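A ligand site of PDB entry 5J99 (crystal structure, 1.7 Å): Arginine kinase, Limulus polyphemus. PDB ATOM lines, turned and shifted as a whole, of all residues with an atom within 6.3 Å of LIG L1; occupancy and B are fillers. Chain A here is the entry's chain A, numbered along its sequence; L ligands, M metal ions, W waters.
OG of Ser 56 sits at hydrogen-bond distance from O of Phe 194, at 2.8 Å.
O of Gly 66 sits at hydrogen-bond distance from N of Gly 57, 3.1 Å away.
OE1 of Glu 225 lies within salt-bridge range of NH2 of Arg 229.
The side-chain carboxylate of Glu 225 sits at hydrogen-bond distance from the side-chain amide nitrogen of Asn 274 (3.3 Å).
OD1 of Asn 274 lies within hydrogen-bond range of NH2 of Arg 126.
Ser 63 touches LIG L1.
Phe 194 touches LIG L1.
OG1 of Thr 273 touches N4 of LIG L1 (3.9 Å).
Asn 274 touches LIG L1 (ND2 to N4, 3.9 Å).
Hydrophobic or aromatic side chains that line LIG L1: Val 65, Tyr 68, Phe 194 and His 315.
Of the 22 residues printed, 12 come within 4 Å of LIG L1.
The nearest printed residue that does not touch LIG L1 is Ser 56 (4.5 Å).
The backbone NH (N) of Glu 314 lies within hydrogen-bond range of an oxygen (O4) of LG2 L2 (2.9 Å).
The side-chain sulfur of Cys 271 lies within hydrogen-bond range of a nitrogen (N4) of LIG L1.
A nitrogen (N3) of LIG L1 lies within salt-bridge range of the side-chain carboxylate of Glu 225 (2.7 Å).
A ring nitrogen (NE2) of His 315 sits at hydrogen-bond distance from an oxygen (O2) of LIG L1 (3.4 Å).
The backbone NH of Val 65 is in hydrogen-bond range of an oxygen (O1) of LIG L1 (2.8 Å).
O4 of LG2 L2 lies within salt-bridge range of NH1 of Arg 309, at 2.8 Å.
OE1 of Glu 314 is in salt-bridge range of N2 of LIG L1.
The side-chain hydroxyl (OH) of Tyr 68 lies within hydrogen-bond range of a nitrogen (N1) of LIG L1 (2.8 Å).
An oxygen (O1) of LG2 L2 is in salt-bridge range of the guanidinium group of Arg 126 (2.6 Å).
N of Gly 64 is in hydrogen-bond range of O2 of LIG L1, at 2.8 Å.
The backbone NH (N) of Gly 66 is in hydrogen-bond range of an oxygen (O1) of LIG L1 (2.8 Å).
NH1 of Arg 229 is in salt-bridge range of O1 of LG2 L2, at 3.8 Å.
Water W3 lies within hydrogen-bond range of OG of Ser 56, OG of Ser 63 and N1 of LIG L1.
Water W2 lies within hydrogen-bond range of the backbone carbonyl oxygen of Ile 67 (2.8 Å), a nitrogen (N1) of LIG L1 (2.8 Å), the side-chain sulfur of Cys 271 (3.2 Å) and the backbone NH of Gly 66 (3.3 Å).
Water W4 lies within hydrogen-bond range of the side-chain hydroxyl (OH) of Tyr 68 (2.6 Å), a nitrogen (N3) of LIG L1 (3.3 Å) and the side-chain carboxylate (OE2) of Glu 225 (3.3 Å).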
ATOM      1  N   SER A  25      19.421  14.769  15.586  1.00  0.00           N
ATOM      2  CA  SER A  25      18.835  13.993  14.496  1.00  0.00           C
ATOM      3  C   SER A  25      17.432  14.487  14.118  1.00  0.00           C
ATOM      4  O   SER A  25      16.790  15.173  14.898  1.00  0.00           O
ATOM      5  CB  SER A  25      18.744  12.526  14.887  1.00  0.00           C
ATOM      6  OG  SER A  25      17.827  12.414  15.950  1.00  0.00           O
ATOM      7  N   SER A  56      17.598   2.320  15.725  1.00  0.00           N
ATOM      8  CA  SER A  56      18.934   2.730  15.293  1.00  0.00           C
ATOM      9  C   SER A  56      19.250   4.159  15.734  1.00  0.00           C
ATOM     10  O   SER A  56      20.388   4.490  16.100  1.00  0.00           O
ATOM     11  CB  SER A  56      19.077   2.614  13.763  1.00  0.00           C
ATOM     12  OG  SER A  56      20.348   3.126  13.279  1.00  0.00           O
ATOM     13  N   GLY A  57      18.228   5.025  15.702  1.00  0.00           N
ATOM     14  CA  GLY A  57      18.402   6.424  16.062  1.00  0.00           C
ATOM     15  C   GLY A  57      18.519   6.584  17.570  1.00  0.00           C
ATOM     16  O   GLY A  57      19.191   7.490  18.065  1.00  0.00           O
ATOM     17  N   ASP A  62      24.530   9.980  17.447  1.00  0.00           N
ATOM     18  CA  ASP A  62      25.137  10.807  16.396  1.00  0.00           C
ATOM     19  C   ASP A  62      24.456  10.621  15.021  1.00  0.00           C
ATOM     20  O   ASP A  62      24.960  11.093  13.993  1.00  0.00           O
ATOM     21  CB  ASP A  62      26.658  10.553  16.305  1.00  0.00           C
ATOM     22  CG  ASP A  62      27.022   9.099  16.023  1.00  0.00           C
ATOM     23  OD1 ASP A  62      26.247   8.231  16.446  1.00  0.00           O
ATOM     24  OD2 ASP A  62      28.066   8.843  15.395  1.00  0.00           O
ATOM     25  N   SER A  63      23.286   9.963  14.987  1.00  0.00           N
ATOM     26  CA  SER A  63      22.471   9.838  13.764  1.00  0.00           C
ATOM     27  C   SER A  63      22.022  11.189  13.242  1.00  0.00           C
ATOM     28  O   SER A  63      21.686  12.085  14.022  1.00  0.00           O
ATOM     29  CB  SER A  63      21.216   8.989  14.015  1.00  0.00           C
ATOM     30  OG  SER A  63      21.541   7.668  14.424  1.00  0.00           O
ATOM     31  N   GLY A  64      21.996  11.324  11.937  1.00  0.00           N
ATOM     32  CA  GLY A  64      21.467  12.540  11.304  1.00  0.00           C
ATOM     33  C   GLY A  64      19.964  12.451  11.042  1.00  0.00           C
ATOM     34  O   GLY A  64      19.242  13.456  11.081  1.00  0.00           O
ATOM     35  N   VAL A  65      19.499  11.211  10.788  1.00  0.00           N
ATOM     36  CA  VAL A  65      18.100  10.948  10.469  1.00  0.00           C
ATOM     37  C   VAL A  65      17.545  10.097  11.590  1.00  0.00           C
ATOM     38  O   VAL A  65      16.786  10.589  12.401  1.00  0.00           O
ATOM     39  CB  VAL A  65      17.951  10.209   9.111  1.00  0.00           C
ATOM     40  CG1 VAL A  65      16.472  10.009   8.786  1.00  0.00           C
ATOM     41  CG2 VAL A  65      18.650  11.029   7.983  1.00  0.00           C
ATOM     42  N   GLY A  66      17.983   8.845  11.649  1.00  0.00           N
ATOM     43  CA  GLY A  66      17.734   7.971  12.801  1.00  0.00           C
ATOM     44  C   GLY A  66      16.527   7.034  12.742  1.00  0.00           C
ATOM     45  O   GLY A  66      16.198   6.385  13.736  1.00  0.00           O
ATOM     46  N   ILE A  67      15.867   6.936  11.570  1.00  0.00           N
ATOM     47  CA  ILE A  67      14.772   5.998  11.424  1.00  0.00           C
ATOM     48  C   ILE A  67      14.952   5.220  10.117  1.00  0.00           C
ATOM     49  O   ILE A  67      15.651   5.700   9.230  1.00  0.00           O
ATOM     50  CB  ILE A  67      13.400   6.663  11.381  1.00  0.00           C
ATOM     51  CG1 ILE A  67      13.265   7.620  10.211  1.00  0.00           C
ATOM     52  CG2 ILE A  67      13.134   7.419  12.671  1.00  0.00           C
ATOM     53  CD1 ILE A  67      11.765   8.106  10.049  1.00  0.00           C
ATOM     54  N   TYR A  68      14.315   4.057  10.057  1.00  0.00           N
ATOM     55  CA  TYR A  68      14.239   3.194   8.869  1.00  0.00           C
ATOM     56  C   TYR A  68      12.862   2.591   8.761  1.00  0.00           C
ATOM     57  O   TYR A  68      12.189   2.481   9.765  1.00  0.00           O
ATOM     58  CB  TYR A  68      15.251   2.052   8.917  1.00  0.00           C
ATOM     59  CG  TYR A  68      16.708   2.473   8.885  1.00  0.00           C
ATOM     60  CD1 TYR A  68      17.377   2.628   7.654  1.00  0.00           C
ATOM     61  CD2 TYR A  68      17.406   2.698  10.054  1.00  0.00           C
ATOM     62  CE1 TYR A  68      18.697   3.021   7.623  1.00  0.00           C
ATOM     63  CE2 TYR A  68      18.750   3.076  10.032  1.00  0.00           C
ATOM     64  CZ  TYR A  68      19.385   3.240   8.811  1.00  0.00           C
ATOM     65  OH  TYR A  68      20.707   3.625   8.768  1.00  0.00           O
ATOM     66  N   ARG A 126      24.342   6.841  -8.420  1.00  0.00           N
ATOM     67  CA  ARG A 126      23.666   5.576  -8.031  1.00  0.00           C
ATOM     68  C   ARG A 126      22.172   5.743  -7.838  1.00  0.00           C
ATOM     69  O   ARG A 126      21.704   6.841  -7.524  1.00  0.00           O
ATOM     70  CB  ARG A 126      24.331   4.977  -6.772  1.00  0.00           C
ATOM     71  CG  ARG A 126      24.208   5.813  -5.466  1.00  0.00           C
ATOM     72  CD  ARG A 126      22.836   5.600  -4.729  1.00  0.00           C
ATOM     73  NE  ARG A 126      22.950   6.074  -3.334  1.00  0.00           N
ATOM     74  CZ  ARG A 126      21.961   6.551  -2.586  1.00  0.00           C
ATOM     75  NH1 ARG A 126      22.209   6.910  -1.310  1.00  0.00           N
ATOM     76  NH2 ARG A 126      20.735   6.660  -3.083  1.00  0.00           N
ATOM     77  N   PHE A 194      25.041   1.854  12.182  1.00  0.00           N
ATOM     78  CA  PHE A 194      23.692   2.364  11.990  1.00  0.00           C
ATOM     79  C   PHE A 194      22.791   1.285  11.443  1.00  0.00           C
ATOM     80  O   PHE A 194      21.668   1.106  11.924  1.00  0.00           O
ATOM     81  CB  PHE A 194      23.740   3.607  11.065  1.00  0.00           C
ATOM     82  CG  PHE A 194      24.606   4.696  11.622  1.00  0.00           C
ATOM     83  CD1 PHE A 194      24.107   5.554  12.621  1.00  0.00           C
ATOM     84  CD2 PHE A 194      25.929   4.837  11.236  1.00  0.00           C
ATOM     85  CE1 PHE A 194      24.903   6.564  13.154  1.00  0.00           C
ATOM     86  CE2 PHE A 194      26.718   5.836  11.758  1.00  0.00           C
ATOM     87  CZ  PHE A 194      26.208   6.703  12.738  1.00  0.00           C
ATOM     88  N   LEU A 195      23.268   0.547  10.437  1.00  0.00           N
ATOM     89  CA  LEU A 195      22.500  -0.557   9.873  1.00  0.00           C
ATOM     90  C   LEU A 195      22.376  -1.717  10.815  1.00  0.00           C
ATOM     91  O   LEU A 195      21.313  -2.349  10.911  1.00  0.00           O
ATOM     92  CB  LEU A 195      23.153  -1.044   8.553  1.00  0.00           C
ATOM     93  CG  LEU A 195      23.032  -0.065   7.397  1.00  0.00           C
ATOM     94  CD1 LEU A 195      23.746  -0.709   6.232  1.00  0.00           C
ATOM     95  CD2 LEU A 195      21.574   0.160   7.054  1.00  0.00           C
ATOM     96  N   GLU A 225      22.048  -1.996   1.911  1.00  0.00           N
ATOM     97  CA  GLU A 225      21.020  -1.197   2.576  1.00  0.00           C
ATOM     98  C   GLU A 225      19.674  -1.392   1.875  1.00  0.00           C
ATOM     99  O   GLU A 225      18.636  -1.588   2.539  1.00  0.00           O
ATOM    100  CB  GLU A 225      21.451   0.280   2.585  1.00  0.00           C
ATOM    101  CG  GLU A 225      20.314   1.162   3.164  1.00  0.00           C
ATOM    102  CD  GLU A 225      20.739   2.596   3.258  1.00  0.00           C
ATOM    103  OE1 GLU A 225      19.844   3.459   3.201  1.00  0.00           O
ATOM    104  OE2 GLU A 225      21.958   2.848   3.406  1.00  0.00           O
ATOM    105  N   ARG A 229      21.419  -1.671  -5.259  1.00  0.00           N
ATOM    106  CA  ARG A 229      21.928  -0.342  -5.607  1.00  0.00           C
ATOM    107  C   ARG A 229      22.583  -0.481  -6.965  1.00  0.00           C
ATOM    108  O   ARG A 229      23.385  -1.382  -7.179  1.00  0.00           O
ATOM    109  CB  ARG A 229      22.940   0.154  -4.602  1.00  0.00           C
ATOM    110  CG  ARG A 229      22.346   0.458  -3.261  1.00  0.00           C
ATOM    111  CD  ARG A 229      21.530   1.760  -3.312  1.00  0.00           C
ATOM    112  NE  ARG A 229      20.987   2.068  -1.978  1.00  0.00           N
ATOM    113  CZ  ARG A 229      21.680   2.723  -1.039  1.00  0.00           C
ATOM    114  NH1 ARG A 229      22.940   3.091  -1.278  1.00  0.00           N
ATOM    115  NH2 ARG A 229      21.104   3.009   0.129  1.00  0.00           N
ATOM    116  N   CYS A 271      15.582   3.533   3.758  1.00  0.00           N
ATOM    117  CA  CYS A 271      15.732   4.800   4.485  1.00  0.00           C
ATOM    118  C   CYS A 271      14.918   5.877   3.731  1.00  0.00           C
ATOM    119  O   CYS A 271      14.977   5.944   2.502  1.00  0.00           O
ATOM    120  CB  CYS A 271      17.221   5.172   4.610  1.00  0.00           C
ATOM    121  SG  CYS A 271      17.767   6.325   5.966  1.00  0.00           S
ATOM    122  N   PRO A 272      14.154   6.723   4.445  1.00  0.00           N
ATOM    123  CA  PRO A 272      13.341   7.740   3.755  1.00  0.00           C
ATOM    124  C   PRO A 272      14.187   8.790   3.004  1.00  0.00           C
ATOM    125  O   PRO A 272      13.629   9.488   2.156  1.00  0.00           O
ATOM    126  CB  PRO A 272      12.540   8.403   4.908  1.00  0.00           C
ATOM    127  CG  PRO A 272      13.339   8.042   6.151  1.00  0.00           C
ATOM    128  CD  PRO A 272      13.868   6.663   5.887  1.00  0.00           C
ATOM    129  N   THR A 273      15.488   8.895   3.269  1.00  0.00           N
ATOM    130  CA  THR A 273      16.262   9.903   2.521  1.00  0.00           C
ATOM    131  C   THR A 273      16.506   9.416   1.101  1.00  0.00           C
ATOM    132  O   THR A 273      16.926  10.191   0.247  1.00  0.00           O
ATOM    133  CB  THR A 273      17.602  10.178   3.151  1.00  0.00           C
ATOM    134  OG1 THR A 273      18.366   8.974   3.130  1.00  0.00           O
ATOM    135  CG2 THR A 273      17.448  10.621   4.620  1.00  0.00           C
ATOM    136  N   ASN A 274      16.242   8.128   0.841  1.00  0.00           N
ATOM    137  CA  ASN A 274      16.459   7.604  -0.494  1.00  0.00           C
ATOM    138  C   ASN A 274      15.199   7.408  -1.353  1.00  0.00           C
ATOM    139  O   ASN A 274      15.285   6.828  -2.418  1.00  0.00           O
ATOM    140  CB  ASN A 274      17.234   6.283  -0.377  1.00  0.00           C
ATOM    141  CG  ASN A 274      18.669   6.548   0.014  1.00  0.00           C
ATOM    142  OD1 ASN A 274      19.281   7.408  -0.558  1.00  0.00           O
ATOM    143  ND2 ASN A 274      19.204   5.817   0.999  1.00  0.00           N
ATOM    144  N   ARG A 309      30.166  14.479   2.334  1.00  0.00           N
ATOM    145  CA  ARG A 309      30.563  13.230   3.027  1.00  0.00           C
ATOM    146  C   ARG A 309      32.075  13.046   2.944  1.00  0.00           C
ATOM    147  O   ARG A 309      32.720  13.673   2.102  1.00  0.00           O
ATOM    148  CB  ARG A 309      29.863  12.021   2.363  1.00  0.00           C
ATOM    149  CG  ARG A 309      28.384  11.986   2.532  1.00  0.00           C
ATOM    150  CD  ARG A 309      27.774  10.782   1.761  1.00  0.00           C
ATOM    151  NE  ARG A 309      26.318  10.879   1.837  1.00  0.00           N
ATOM    152  CZ  ARG A 309      25.472   9.864   1.694  1.00  0.00           C
ATOM    153  NH1 ARG A 309      25.956   8.633   1.495  1.00  0.00           N
ATOM    154  NH2 ARG A 309      24.176  10.084   1.812  1.00  0.00           N
ATOM    155  N   GLU A 314      29.621   8.165   3.787  1.00  0.00           N
ATOM    156  CA  GLU A 314      29.051   8.892   4.938  1.00  0.00           C
ATOM    157  C   GLU A 314      29.676   8.422   6.261  1.00  0.00           C
ATOM    158  O   GLU A 314      30.127   7.262   6.372  1.00  0.00           O
ATOM    159  CB  GLU A 314      27.539   8.704   4.996  1.00  0.00           C
ATOM    160  CG  GLU A 314      27.168   7.218   4.929  1.00  0.00           C
ATOM    161  CD  GLU A 314      25.665   7.009   5.196  1.00  0.00           C
ATOM    162  OE1 GLU A 314      24.945   8.040   5.389  1.00  0.00           O
ATOM    163  OE2 GLU A 314      25.235   5.835   5.194  1.00  0.00           O
ATOM    164  N   HIS A 315      29.645   9.317   7.257  1.00  0.00           N
ATOM    165  CA  HIS A 315      30.275   9.070   8.547  1.00  0.00           C
ATOM    166  C   HIS A 315      31.762   8.745   8.455  1.00  0.00           C
ATOM    167  O   HIS A 315      32.288   8.016   9.298  1.00  0.00           O
ATOM    168  CB  HIS A 315      29.557   7.932   9.292  1.00  0.00           C
ATOM    169  CG  HIS A 315      28.069   8.088   9.312  1.00  0.00           C
ATOM    170  ND1 HIS A 315      27.221   7.176   8.708  1.00  0.00           N
ATOM    171  CD2 HIS A 315      27.269   9.036   9.865  1.00  0.00           C
ATOM    172  CE1 HIS A 315      25.971   7.559   8.878  1.00  0.00           C
ATOM    173  NE2 HIS A 315      25.975   8.686   9.570  1.00  0.00           N
HETATM  174  N1  LIG L   1      20.901   6.112  10.009  1.00  0.00           N
HETATM  175  C1  LIG L   1      21.998   7.001   9.654  1.00  0.00           C
HETATM  176  C2  LIG L   1      21.763   8.384  10.246  1.00  0.00           C
HETATM  177  O1  LIG L   1      20.702   8.640  10.833  1.00  0.00           O
HETATM  178  C3  LIG L   1      22.158   7.087   8.129  1.00  0.00           C
HETATM  179  C4  LIG L   1      20.977   7.741   7.428  1.00  0.00           C
HETATM  180  C5  LIG L   1      21.328   8.300   6.080  1.00  0.00           C
HETATM  181  N2  LIG L   1      22.080   7.320   5.310  1.00  0.00           N
HETATM  182  C6  LIG L   1      21.544   6.256   4.701  1.00  0.00           C
HETATM  183  N3  LIG L   1      22.344   5.411   4.060  1.00  0.00           N
HETATM  184  N4  LIG L   1      20.236   5.995   4.790  1.00  0.00           N
HETATM  185  O2  LIG L   1      22.642   9.236  10.148  1.00  0.00           O
HETATM  186  P1  LG2 L   2      25.872   5.374  -1.105  1.00  0.00           P
HETATM  187  O1  LG2 L   2      24.764   6.373  -1.035  1.00  0.00           O
HETATM  188  O2  LG2 L   2      26.152   4.864  -2.506  1.00  0.00           O
HETATM  189  O3  LG2 L   2      25.576   4.116  -0.284  1.00  0.00           O
HETATM  190  P2  LG2 L   2      28.149   5.906   0.719  1.00  0.00           P
HETATM  191  O4  LG2 L   2      28.408   7.256   1.350  1.00  0.00           O
HETATM  192  O5  LG2 L   2      27.603   4.750   1.592  1.00  0.00           O
HETATM  193  O6  LG2 L   2      27.187   6.111  -0.561  1.00  0.00           O
HETATM  194  O7  LG2 L   2      29.535   5.554   0.035  1.00  0.00           O
HETATM  195  C1  LG2 L   2      29.606   4.332  -0.736  1.00  0.00           C
HETATM  196  C2  LG2 L   2      30.929   4.229  -1.474  1.00  0.00           C
HETATM  197  O8  LG2 L   2      30.889   5.066  -2.644  1.00  0.00           O
HETATM  198  C3  LG2 L   2      32.134   4.644  -0.661  1.00  0.00           C
HETATM  199  O9  LG2 L   2      33.234   3.754  -0.880  1.00  0.00           O
HETATM  200  C4  LG2 L   2      32.512   5.995  -1.265  1.00  0.00           C
HETATM  201  O10 LG2 L   2      33.898   6.229  -1.193  1.00  0.00           O
HETATM  202  C5  LG2 L   2      32.110   5.788  -2.691  1.00  0.00           C
HETATM  203  N1  LG2 L   2      31.864   7.006  -3.482  1.00  0.00           N
HETATM  204  C6  LG2 L   2      30.828   7.870  -3.333  1.00  0.00           C
HETATM  205  N2  LG2 L   2      30.936   8.832  -4.310  1.00  0.00           N
HETATM  206  C7  LG2 L   2      32.053   8.564  -5.027  1.00  0.00           C
HETATM  207  C8  LG2 L   2      32.742   9.195  -6.169  1.00  0.00           C
HETATM  208  N3  LG2 L   2      32.253  10.321  -6.740  1.00  0.00           N
HETATM  209  N4  LG2 L   2      33.847   8.582  -6.616  1.00  0.00           N
HETATM  210  C9  LG2 L   2      34.386   7.473  -6.081  1.00  0.00           C
HETATM  211  N5  LG2 L   2      33.803   6.863  -5.043  1.00  0.00           N
HETATM  212  C10 LG2 L   2      32.665   7.371  -4.479  1.00  0.00           C
HETATM  213 MG    MG M   1      25.843   3.634   1.656  1.00  0.00          MG
HETATM  214  O   HOH W   1      22.229  11.133   7.305  1.00  0.00           O
HETATM  215  O   HOH W   2      18.266   6.707   9.102  1.00  0.00           O
HETATM  216  O   HOH W   3      20.462   5.773  12.761  1.00  0.00           O
HETATM  217  O   HOH W   4      22.226   3.463   6.681  1.00  0.00           O
